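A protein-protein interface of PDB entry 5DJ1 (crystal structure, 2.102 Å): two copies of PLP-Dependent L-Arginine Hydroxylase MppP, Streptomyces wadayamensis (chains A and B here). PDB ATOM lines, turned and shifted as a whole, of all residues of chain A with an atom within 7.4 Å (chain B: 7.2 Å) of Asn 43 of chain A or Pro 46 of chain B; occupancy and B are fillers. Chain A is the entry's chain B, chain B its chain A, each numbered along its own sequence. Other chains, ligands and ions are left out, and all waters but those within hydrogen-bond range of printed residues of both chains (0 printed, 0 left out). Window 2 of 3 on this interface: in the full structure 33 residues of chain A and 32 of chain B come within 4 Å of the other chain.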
ATOM      1  N   LEU A  34     -17.662  -3.402 -12.114  1.00  0.00           N
ATOM      2  CA  LEU A  34     -16.950  -2.961 -13.302  1.00  0.00           C
ATOM      3  C   LEU A  34     -17.528  -1.649 -13.837  1.00  0.00           C
ATOM      4  O   LEU A  34     -18.739  -1.440 -13.834  1.00  0.00           O
ATOM      5  CB  LEU A  34     -17.071  -4.039 -14.390  1.00  0.00           C
ATOM      6  CG  LEU A  34     -16.421  -5.399 -14.141  1.00  0.00           C
ATOM      7  CD1 LEU A  34     -16.943  -6.416 -15.111  1.00  0.00           C
ATOM      8  CD2 LEU A  34     -14.930  -5.281 -14.296  1.00  0.00           C
ATOM      9  N   PRO A  36     -18.217   0.767 -17.281  1.00  0.00           N
ATOM     10  CA  PRO A  36     -18.586   0.386 -18.655  1.00  0.00           C
ATOM     11  C   PRO A  36     -17.384   0.045 -19.527  1.00  0.00           C
ATOM     12  O   PRO A  36     -17.455  -0.884 -20.324  1.00  0.00           O
ATOM     13  CB  PRO A  36     -19.349   1.628 -19.176  1.00  0.00           C
ATOM     14  CG  PRO A  36     -19.805   2.352 -17.954  1.00  0.00           C
ATOM     15  CD  PRO A  36     -18.743   2.096 -16.909  1.00  0.00           C
ATOM     16  N   GLN A  38     -14.470  -1.240 -18.530  1.00  0.00           N
ATOM     17  CA  GLN A  38     -13.977  -2.539 -18.073  1.00  0.00           C
ATOM     18  C   GLN A  38     -14.931  -3.655 -18.437  1.00  0.00           C
ATOM     19  O   GLN A  38     -14.506  -4.759 -18.787  1.00  0.00           O
ATOM     20  CB  GLN A  38     -13.769  -2.527 -16.549  1.00  0.00           C
ATOM     21  CG  GLN A  38     -12.734  -1.546 -16.143  1.00  0.00           C
ATOM     22  CD  GLN A  38     -12.743  -1.231 -14.655  1.00  0.00           C
ATOM     23  OE1 GLN A  38     -13.725  -1.454 -13.933  1.00  0.00           O
ATOM     24  NE2 GLN A  38     -11.641  -0.701 -14.202  1.00  0.00           N
ATOM     25  N   GLN A  39     -16.222  -3.400 -18.316  1.00  0.00           N
ATOM     26  CA  GLN A  39     -17.207  -4.423 -18.631  1.00  0.00           C
ATOM     27  C   GLN A  39     -17.186  -4.790 -20.112  1.00  0.00           C
ATOM     28  O   GLN A  39     -17.376  -5.957 -20.470  1.00  0.00           O
ATOM     29  CB  GLN A  39     -18.584  -3.932 -18.236  1.00  0.00           C
ATOM     30  CG  GLN A  39     -19.634  -5.022 -18.261  1.00  0.00           C
ATOM     31  CD  GLN A  39     -20.677  -4.726 -17.228  1.00  0.00           C
ATOM     32  OE1 GLN A  39     -21.278  -3.634 -17.238  1.00  0.00           O
ATOM     33  NE2 GLN A  39     -20.865  -5.658 -16.286  1.00  0.00           N
ATOM     34  N   LYS A  40     -16.929  -3.812 -20.980  1.00  0.00           N
ATOM     35  CA  LYS A  40     -16.701  -4.105 -22.393  1.00  0.00           C
ATOM     36  C   LYS A  40     -15.554  -5.105 -22.597  1.00  0.00           C
ATOM     37  O   LYS A  40     -15.627  -6.011 -23.448  1.00  0.00           O
ATOM     38  CB  LYS A  40     -16.409  -2.803 -23.134  1.00  0.00           C
ATOM     39  CG  LYS A  40     -16.444  -2.967 -24.651  1.00  0.00           C
ATOM     40  CD  LYS A  40     -16.118  -1.676 -25.360  1.00  0.00           C
ATOM     41  CE  LYS A  40     -16.047  -1.872 -26.872  1.00  0.00           C
ATOM     42  NZ  LYS A  40     -14.862  -2.712 -27.236  1.00  0.00           N
ATOM     43  N   ILE A  41     -14.476  -4.951 -21.836  1.00  0.00           N
ATOM     44  CA  ILE A  41     -13.355  -5.877 -21.949  1.00  0.00           C
ATOM     45  C   ILE A  41     -13.778  -7.285 -21.532  1.00  0.00           C
ATOM     46  O   ILE A  41     -13.437  -8.278 -22.186  1.00  0.00           O
ATOM     47  CB  ILE A  41     -12.179  -5.367 -21.105  1.00  0.00           C
ATOM     48  CG1 ILE A  41     -11.670  -4.034 -21.678  1.00  0.00           C
ATOM     49  CG2 ILE A  41     -11.080  -6.426 -21.040  1.00  0.00           C
ATOM     50  CD1 ILE A  41     -10.787  -3.239 -20.736  1.00  0.00           C
ATOM     51  N   VAL A  42     -14.510  -7.393 -20.425  1.00  0.00           N
ATOM     52  CA  VAL A  42     -14.927  -8.691 -19.917  1.00  0.00           C
ATOM     53  C   VAL A  42     -15.815  -9.389 -20.926  1.00  0.00           C
ATOM     54  O   VAL A  42     -15.700 -10.601 -21.153  1.00  0.00           O
ATOM     55  CB  VAL A  42     -15.632  -8.522 -18.557  1.00  0.00           C
ATOM     56  CG1 VAL A  42     -16.388  -9.774 -18.152  1.00  0.00           C
ATOM     57  CG2 VAL A  42     -14.614  -8.134 -17.482  1.00  0.00           C
ATOM     58  N   ASN A  43     -16.724  -8.650 -21.541  1.00  0.00           N
ATOM     59  CA  ASN A  43     -17.601  -9.302 -22.498  1.00  0.00           C
ATOM     60  C   ASN A  43     -16.874  -9.693 -23.777  1.00  0.00           C
ATOM     61  O   ASN A  43     -17.415 -10.464 -24.554  1.00  0.00           O
ATOM     62  CB  ASN A  43     -18.814  -8.398 -22.747  1.00  0.00           C
ATOM     63  CG  ASN A  43     -19.735  -8.393 -21.545  1.00  0.00           C
ATOM     64  OD1 ASN A  43     -20.340  -9.416 -21.229  1.00  0.00           O
ATOM     65  ND2 ASN A  43     -19.771  -7.291 -20.820  1.00  0.00           N
ATOM     66  N   GLU A  44     -15.637  -9.245 -23.968  1.00  0.00           N
ATOM     67  CA  GLU A  44     -14.807  -9.662 -25.081  1.00  0.00           C
ATOM     68  C   GLU A  44     -13.743 -10.668 -24.666  1.00  0.00           C
ATOM     69  O   GLU A  44     -12.790 -10.900 -25.418  1.00  0.00           O
ATOM     70  CB  GLU A  44     -14.171  -8.429 -25.725  1.00  0.00           C
ATOM     71  CG  GLU A  44     -15.210  -7.628 -26.490  1.00  0.00           C
ATOM     72  CD  GLU A  44     -14.681  -6.325 -27.040  1.00  0.00           C
ATOM     73  OE1 GLU A  44     -13.500  -6.281 -27.446  1.00  0.00           O
ATOM     74  OE2 GLU A  44     -15.471  -5.354 -27.075  1.00  0.00           O
ATOM     75  N   LEU A  45     -13.907 -11.288 -23.503  1.00  0.00           N
ATOM     76  CA  LEU A  45     -12.930 -12.276 -23.055  1.00  0.00           C
ATOM     77  C   LEU A  45     -12.706 -13.412 -24.052  1.00  0.00           C
ATOM     78  O   LEU A  45     -11.541 -13.800 -24.240  1.00  0.00           O
ATOM     79  CB  LEU A  45     -13.348 -12.842 -21.693  1.00  0.00           C
ATOM     80  CG  LEU A  45     -12.666 -12.221 -20.476  1.00  0.00           C
ATOM     81  CD1 LEU A  45     -13.269 -12.788 -19.198  1.00  0.00           C
ATOM     82  CD2 LEU A  45     -11.144 -12.443 -20.491  1.00  0.00           C
ATOM     83  N   PRO A  46     -13.722 -13.982 -24.707  1.00  0.00           N
ATOM     84  CA  PRO A  46     -13.426 -14.980 -25.765  1.00  0.00           C
ATOM     85  C   PRO A  46     -12.521 -14.446 -26.873  1.00  0.00           C
ATOM     86  O   PRO A  46     -11.768 -15.229 -27.466  1.00  0.00           O
ATOM     87  CB  PRO A  46     -14.807 -15.356 -26.309  1.00  0.00           C
ATOM     88  CG  PRO A  46     -15.771 -14.982 -25.251  1.00  0.00           C
ATOM     89  CD  PRO A  46     -15.169 -13.785 -24.527  1.00  0.00           C
ATOM     90  N   VAL A  47     -12.534 -13.134 -27.130  1.00  0.00           N
ATOM     91  CA  VAL A  47     -11.663 -12.564 -28.155  1.00  0.00           C
ATOM     92  C   VAL A  47     -10.233 -12.497 -27.660  1.00  0.00           C
ATOM     93  O   VAL A  47      -9.287 -12.765 -28.413  1.00  0.00           O
ATOM     94  CB  VAL A  47     -12.153 -11.162 -28.586  1.00  0.00           C
ATOM     95  CG1 VAL A  47     -11.312 -10.626 -29.757  1.00  0.00           C
ATOM     96  CG2 VAL A  47     -13.617 -11.203 -28.943  1.00  0.00           C
ATOM     97  N   ILE B  41     -17.166 -23.583 -23.603  1.00  0.00           N
ATOM     98  CA  ILE B  41     -16.861 -23.013 -22.286  1.00  0.00           C
ATOM     99  C   ILE B  41     -16.220 -21.635 -22.436  1.00  0.00           C
ATOM    100  O   ILE B  41     -16.547 -20.682 -21.712  1.00  0.00           O
ATOM    101  CB  ILE B  41     -15.951 -23.979 -21.494  1.00  0.00           C
ATOM    102  CG1 ILE B  41     -16.694 -25.297 -21.218  1.00  0.00           C
ATOM    103  CG2 ILE B  41     -15.442 -23.318 -20.189  1.00  0.00           C
ATOM    104  CD1 ILE B  41     -15.790 -26.431 -20.797  1.00  0.00           C
ATOM    105  N   VAL B  42     -15.263 -21.518 -23.357  1.00  0.00           N
ATOM    106  CA  VAL B  42     -14.589 -20.241 -23.596  1.00  0.00           C
ATOM    107  C   VAL B  42     -15.597 -19.173 -24.007  1.00  0.00           C
ATOM    108  O   VAL B  42     -15.547 -18.031 -23.531  1.00  0.00           O
ATOM    109  CB  VAL B  42     -13.487 -20.422 -24.659  1.00  0.00           C
ATOM    110  CG1 VAL B  42     -12.952 -19.060 -25.166  1.00  0.00           C
ATOM    111  CG2 VAL B  42     -12.376 -21.316 -24.111  1.00  0.00           C
ATOM    112  N   ASN B  43     -16.529 -19.526 -24.895  1.00  0.00           N
ATOM    113  CA  ASN B  43     -17.562 -18.583 -25.311  1.00  0.00           C
ATOM    114  C   ASN B  43     -18.457 -18.168 -24.149  1.00  0.00           C
ATOM    115  O   ASN B  43     -19.059 -17.092 -24.202  1.00  0.00           O
ATOM    116  CB  ASN B  43     -18.402 -19.182 -26.445  1.00  0.00           C
ATOM    117  CG  ASN B  43     -17.605 -19.376 -27.733  1.00  0.00           C
ATOM    118  OD1 ASN B  43     -16.563 -18.758 -27.935  1.00  0.00           O
ATOM    119  ND2 ASN B  43     -18.096 -20.242 -28.601  1.00  0.00           N
ATOM    120  N   GLU B  44     -18.505 -18.943 -23.070  1.00  0.00           N
ATOM    121  CA  GLU B  44     -19.312 -18.591 -21.909  1.00  0.00           C
ATOM    122  C   GLU B  44     -18.545 -17.829 -20.827  1.00  0.00           C
ATOM    123  O   GLU B  44     -19.087 -17.619 -19.737  1.00  0.00           O
ATOM    124  CB  GLU B  44     -19.913 -19.858 -21.296  1.00  0.00           C
ATOM    125  CG  GLU B  44     -21.046 -20.442 -22.129  1.00  0.00           C
ATOM    126  CD  GLU B  44     -21.530 -21.780 -21.585  1.00  0.00           C
ATOM    127  OE1 GLU B  44     -21.071 -22.174 -20.488  1.00  0.00           O
ATOM    128  OE2 GLU B  44     -22.364 -22.437 -22.252  1.00  0.00           O
ATOM    129  N   LEU B  45     -17.300 -17.440 -21.076  1.00  0.00           N
ATOM    130  CA  LEU B  45     -16.534 -16.739 -20.051  1.00  0.00           C
ATOM    131  C   LEU B  45     -17.270 -15.536 -19.485  1.00  0.00           C
ATOM    132  O   LEU B  45     -17.232 -15.341 -18.261  1.00  0.00           O
ATOM    133  CB  LEU B  45     -15.172 -16.330 -20.625  1.00  0.00           C
ATOM    134  CG  LEU B  45     -14.147 -17.471 -20.532  1.00  0.00           C
ATOM    135  CD1 LEU B  45     -12.929 -17.173 -21.370  1.00  0.00           C
ATOM    136  CD2 LEU B  45     -13.751 -17.741 -19.092  1.00  0.00           C
ATOM    137  N   PRO B  46     -17.965 -14.724 -20.276  1.00  0.00           N
ATOM    138  CA  PRO B  46     -18.703 -13.595 -19.675  1.00  0.00           C
ATOM    139  C   PRO B  46     -19.756 -14.046 -18.668  1.00  0.00           C
ATOM    140  O   PRO B  46     -19.989 -13.357 -17.671  1.00  0.00           O
ATOM    141  CB  PRO B  46     -19.318 -12.893 -20.891  1.00  0.00           C
ATOM    142  CG  PRO B  46     -18.492 -13.302 -22.069  1.00  0.00           C
ATOM    143  CD  PRO B  46     -17.957 -14.691 -21.744  1.00  0.00           C
ATOM    144  N   VAL B  47     -20.407 -15.184 -18.914  1.00  0.00           N
ATOM    145  CA  VAL B  47     -21.364 -15.735 -17.955  1.00  0.00           C
ATOM    146  C   VAL B  47     -20.651 -16.297 -16.724  1.00  0.00           C
ATOM    147  O   VAL B  47     -21.128 -16.150 -15.589  1.00  0.00           O
ATOM    148  CB  VAL B  47     -22.224 -16.818 -18.627  1.00  0.00           C
ATOM    149  CG1 VAL B  47     -23.182 -17.459 -17.597  1.00  0.00           C
ATOM    150  CG2 VAL B  47     -22.987 -16.226 -19.854  1.00  0.00           C
ATOM    151  N   LEU B  48     -19.532 -16.994 -16.925  1.00  0.00           N
ATOM    152  CA  LEU B  48     -18.779 -17.471 -15.774  1.00  0.00           C
ATOM    153  C   LEU B  48     -18.261 -16.309 -14.944  1.00  0.00           C
ATOM    154  O   LEU B  48     -18.204 -16.413 -13.716  1.00  0.00           O
ATOM    155  CB  LEU B  48     -17.627 -18.368 -16.219  1.00  0.00           C
ATOM    156  CG  LEU B  48     -18.022 -19.625 -16.991  1.00  0.00           C
ATOM    157  CD1 LEU B  48     -16.775 -20.304 -17.496  1.00  0.00           C
ATOM    158  CD2 LEU B  48     -18.837 -20.567 -16.118  1.00  0.00           C
ATOM    159  N   TRP B  49     -17.898 -15.194 -15.588  1.00  0.00           N
ATOM    160  CA  TRP B  49     -17.531 -13.987 -14.841  1.00  0.00           C
ATOM    161  C   TRP B  49     -18.692 -13.498 -13.977  1.00  0.00           C
ATOM    162  O   TRP B  49     -18.515 -13.218 -12.787  1.00  0.00           O
ATOM    163  CB  TRP B  49     -17.087 -12.866 -15.787  1.00  0.00           C
ATOM    164  CG  TRP B  49     -16.402 -11.728 -15.074  1.00  0.00           C
ATOM    165  CD1 TRP B  49     -16.986 -10.827 -14.213  1.00  0.00           C
ATOM    166  CD2 TRP B  49     -15.026 -11.335 -15.177  1.00  0.00           C
ATOM    167  NE1 TRP B  49     -16.056  -9.914 -13.779  1.00  0.00           N
ATOM    168  CE2 TRP B  49     -14.846 -10.204 -14.343  1.00  0.00           C
ATOM    169  CE3 TRP B  49     -13.928 -11.828 -15.882  1.00  0.00           C
ATOM    170  CZ2 TRP B  49     -13.609  -9.568 -14.190  1.00  0.00           C
ATOM    171  CZ3 TRP B  49     -12.693 -11.194 -15.734  1.00  0.00           C
ATOM    172  CH2 TRP B  49     -12.551 -10.065 -14.897  1.00  0.00           C
ATOM    173  N   ALA B  50     -19.895 -13.398 -14.569  1.00  0.00           N
ATOM    174  CA  ALA B  50     -21.070 -12.963 -13.818  1.00  0.00           C
ATOM    175  C   ALA B  50     -21.291 -13.838 -12.601  1.00  0.00           C
ATOM    176  O   ALA B  50     -21.518 -13.337 -11.489  1.00  0.00           O
ATOM    177  CB  ALA B  50     -22.326 -12.990 -14.705  1.00  0.00           C
ATOM    178  N   GLU B  51     -21.240 -15.157 -12.795  1.00  0.00           N
ATOM    179  CA  GLU B  51     -21.396 -16.088 -11.686  1.00  0.00           C
ATOM    180  C   GLU B  51     -20.292 -15.910 -10.645  1.00  0.00           C
ATOM    181  O   GLU B  51     -20.549 -15.990  -9.439  1.00  0.00           O
ATOM    182  CB  GLU B  51     -21.409 -17.532 -12.214  1.00  0.00           C
ATOM    183  CG  GLU B  51     -21.493 -18.590 -11.094  1.00  0.00           C
ATOM    184  CD  GLU B  51     -21.145 -20.015 -11.537  1.00  0.00           C
ATOM    185  OE1 GLU B  51     -20.789 -20.226 -12.726  1.00  0.00           O
ATOM    186  OE2 GLU B  51     -21.188 -20.918 -10.669  1.00  0.00           O
ATOM    187  N   SER B  52     -19.053 -15.691 -11.087  1.00  0.00           N
ATOM    188  CA  SER B  52     -17.936 -15.575 -10.146  1.00  0.00           C
ATOM    189  C   SER B  52     -18.007 -14.283  -9.337  1.00  0.00           C
ATOM    190  O   SER B  52     -17.511 -14.237  -8.196  1.00  0.00           O
ATOM    191  CB  SER B  52     -16.591 -15.656 -10.887  1.00  0.00           C
ATOM    192  OG  SER B  52     -16.381 -16.928 -11.499  1.00  0.00           O
ATOM    193  N   LEU B 257     -12.979 -17.280 -11.260  1.00  0.00           N
ATOM    194  CA  LEU B 257     -13.122 -17.554 -12.688  1.00  0.00           C
ATOM    195  C   LEU B 257     -12.299 -18.763 -13.105  1.00  0.00           C
ATOM    196  O   LEU B 257     -12.746 -19.586 -13.910  1.00  0.00           O
ATOM    197  CB  LEU B 257     -12.716 -16.344 -13.519  1.00  0.00           C
ATOM    198  CG  LEU B 257     -13.080 -16.505 -14.994  1.00  0.00           C
ATOM    199  CD1 LEU B 257     -14.586 -16.390 -15.157  1.00  0.00           C
ATOM    200  CD2 LEU B 257     -12.416 -15.464 -15.856  1.00  0.00           C
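The backbone carbonyl oxygen (O) of Gln 39 of chain A is in hydrogen-bond range of the side-chain amide nitrogen (ND2) of Asn 43 of chain A (2.8 Å).
Printed residues of chain A that touch a printed residue of chain B: Leu 34, Val 42, Asn 43, Leu 45 and Pro 46.
Hydrophobic or aromatic side chains of chain A within 4 Å of the printed part of chain B: Leu 34, Val 42, Leu 45 and Pro 46.
Of the printed residues of chain B, Asn 43 of chain A touches Pro 46 (3.6 Å).
Printed residues of chain B within 4 Å of Leu 34 of chain A: Trp 49 (3.8 Å).
Printed residues of chain B within 4 Å of Pro 46 of chain A: Val 42.
Of the printed residues of chain B, Leu 45 of chain A touches Trp 49.
Of the printed residues of chain B, Val 42 of chain A touches Pro 46 and Trp 49.
Of the printed residues of chain A, Trp 49 of chain B touches Leu 34 (3.8 Å), Val 42 (3.6 Å) and Leu 45 (3.5 Å).
Glu 44 of chain B touches none of the printed residues of chain A.
The nearest residue of chain B that does not touch Asn 43 of chain A is Val 47 of chain B (6.2 Å).
Leu 34 of chain A touches Trp 49 of chain B (CD1 to NE1, 3.8 Å).
Val 42 of chain A touches Pro 46 of chain B (O to CG, 3.99 Å).
Trp 49 of chain B touches Val 42 of chain A (CD2 to CG1, 3.6 Å).
Pro 46 of chain B touches Asn 43 of chain A.
CE3 of Trp 49 of chain B touches CD1 of Leu 45 of chain A, at 3.5 Å.
Val 42 of chain B touches Pro 46 of chain A (O to CG, 3.5 Å).
Val 42 of chain A touches Pro 46 of chain B, and with the chains exchanged Pro 46 of chain A touches Val 42 of chain B.
Asn 43 of chain A touches Pro 46 of chain B, but with the chains exchanged Pro 46 of chain A does not touch Asn 43 of chain B (4.02 Å).
7 positions are printed for both chains.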
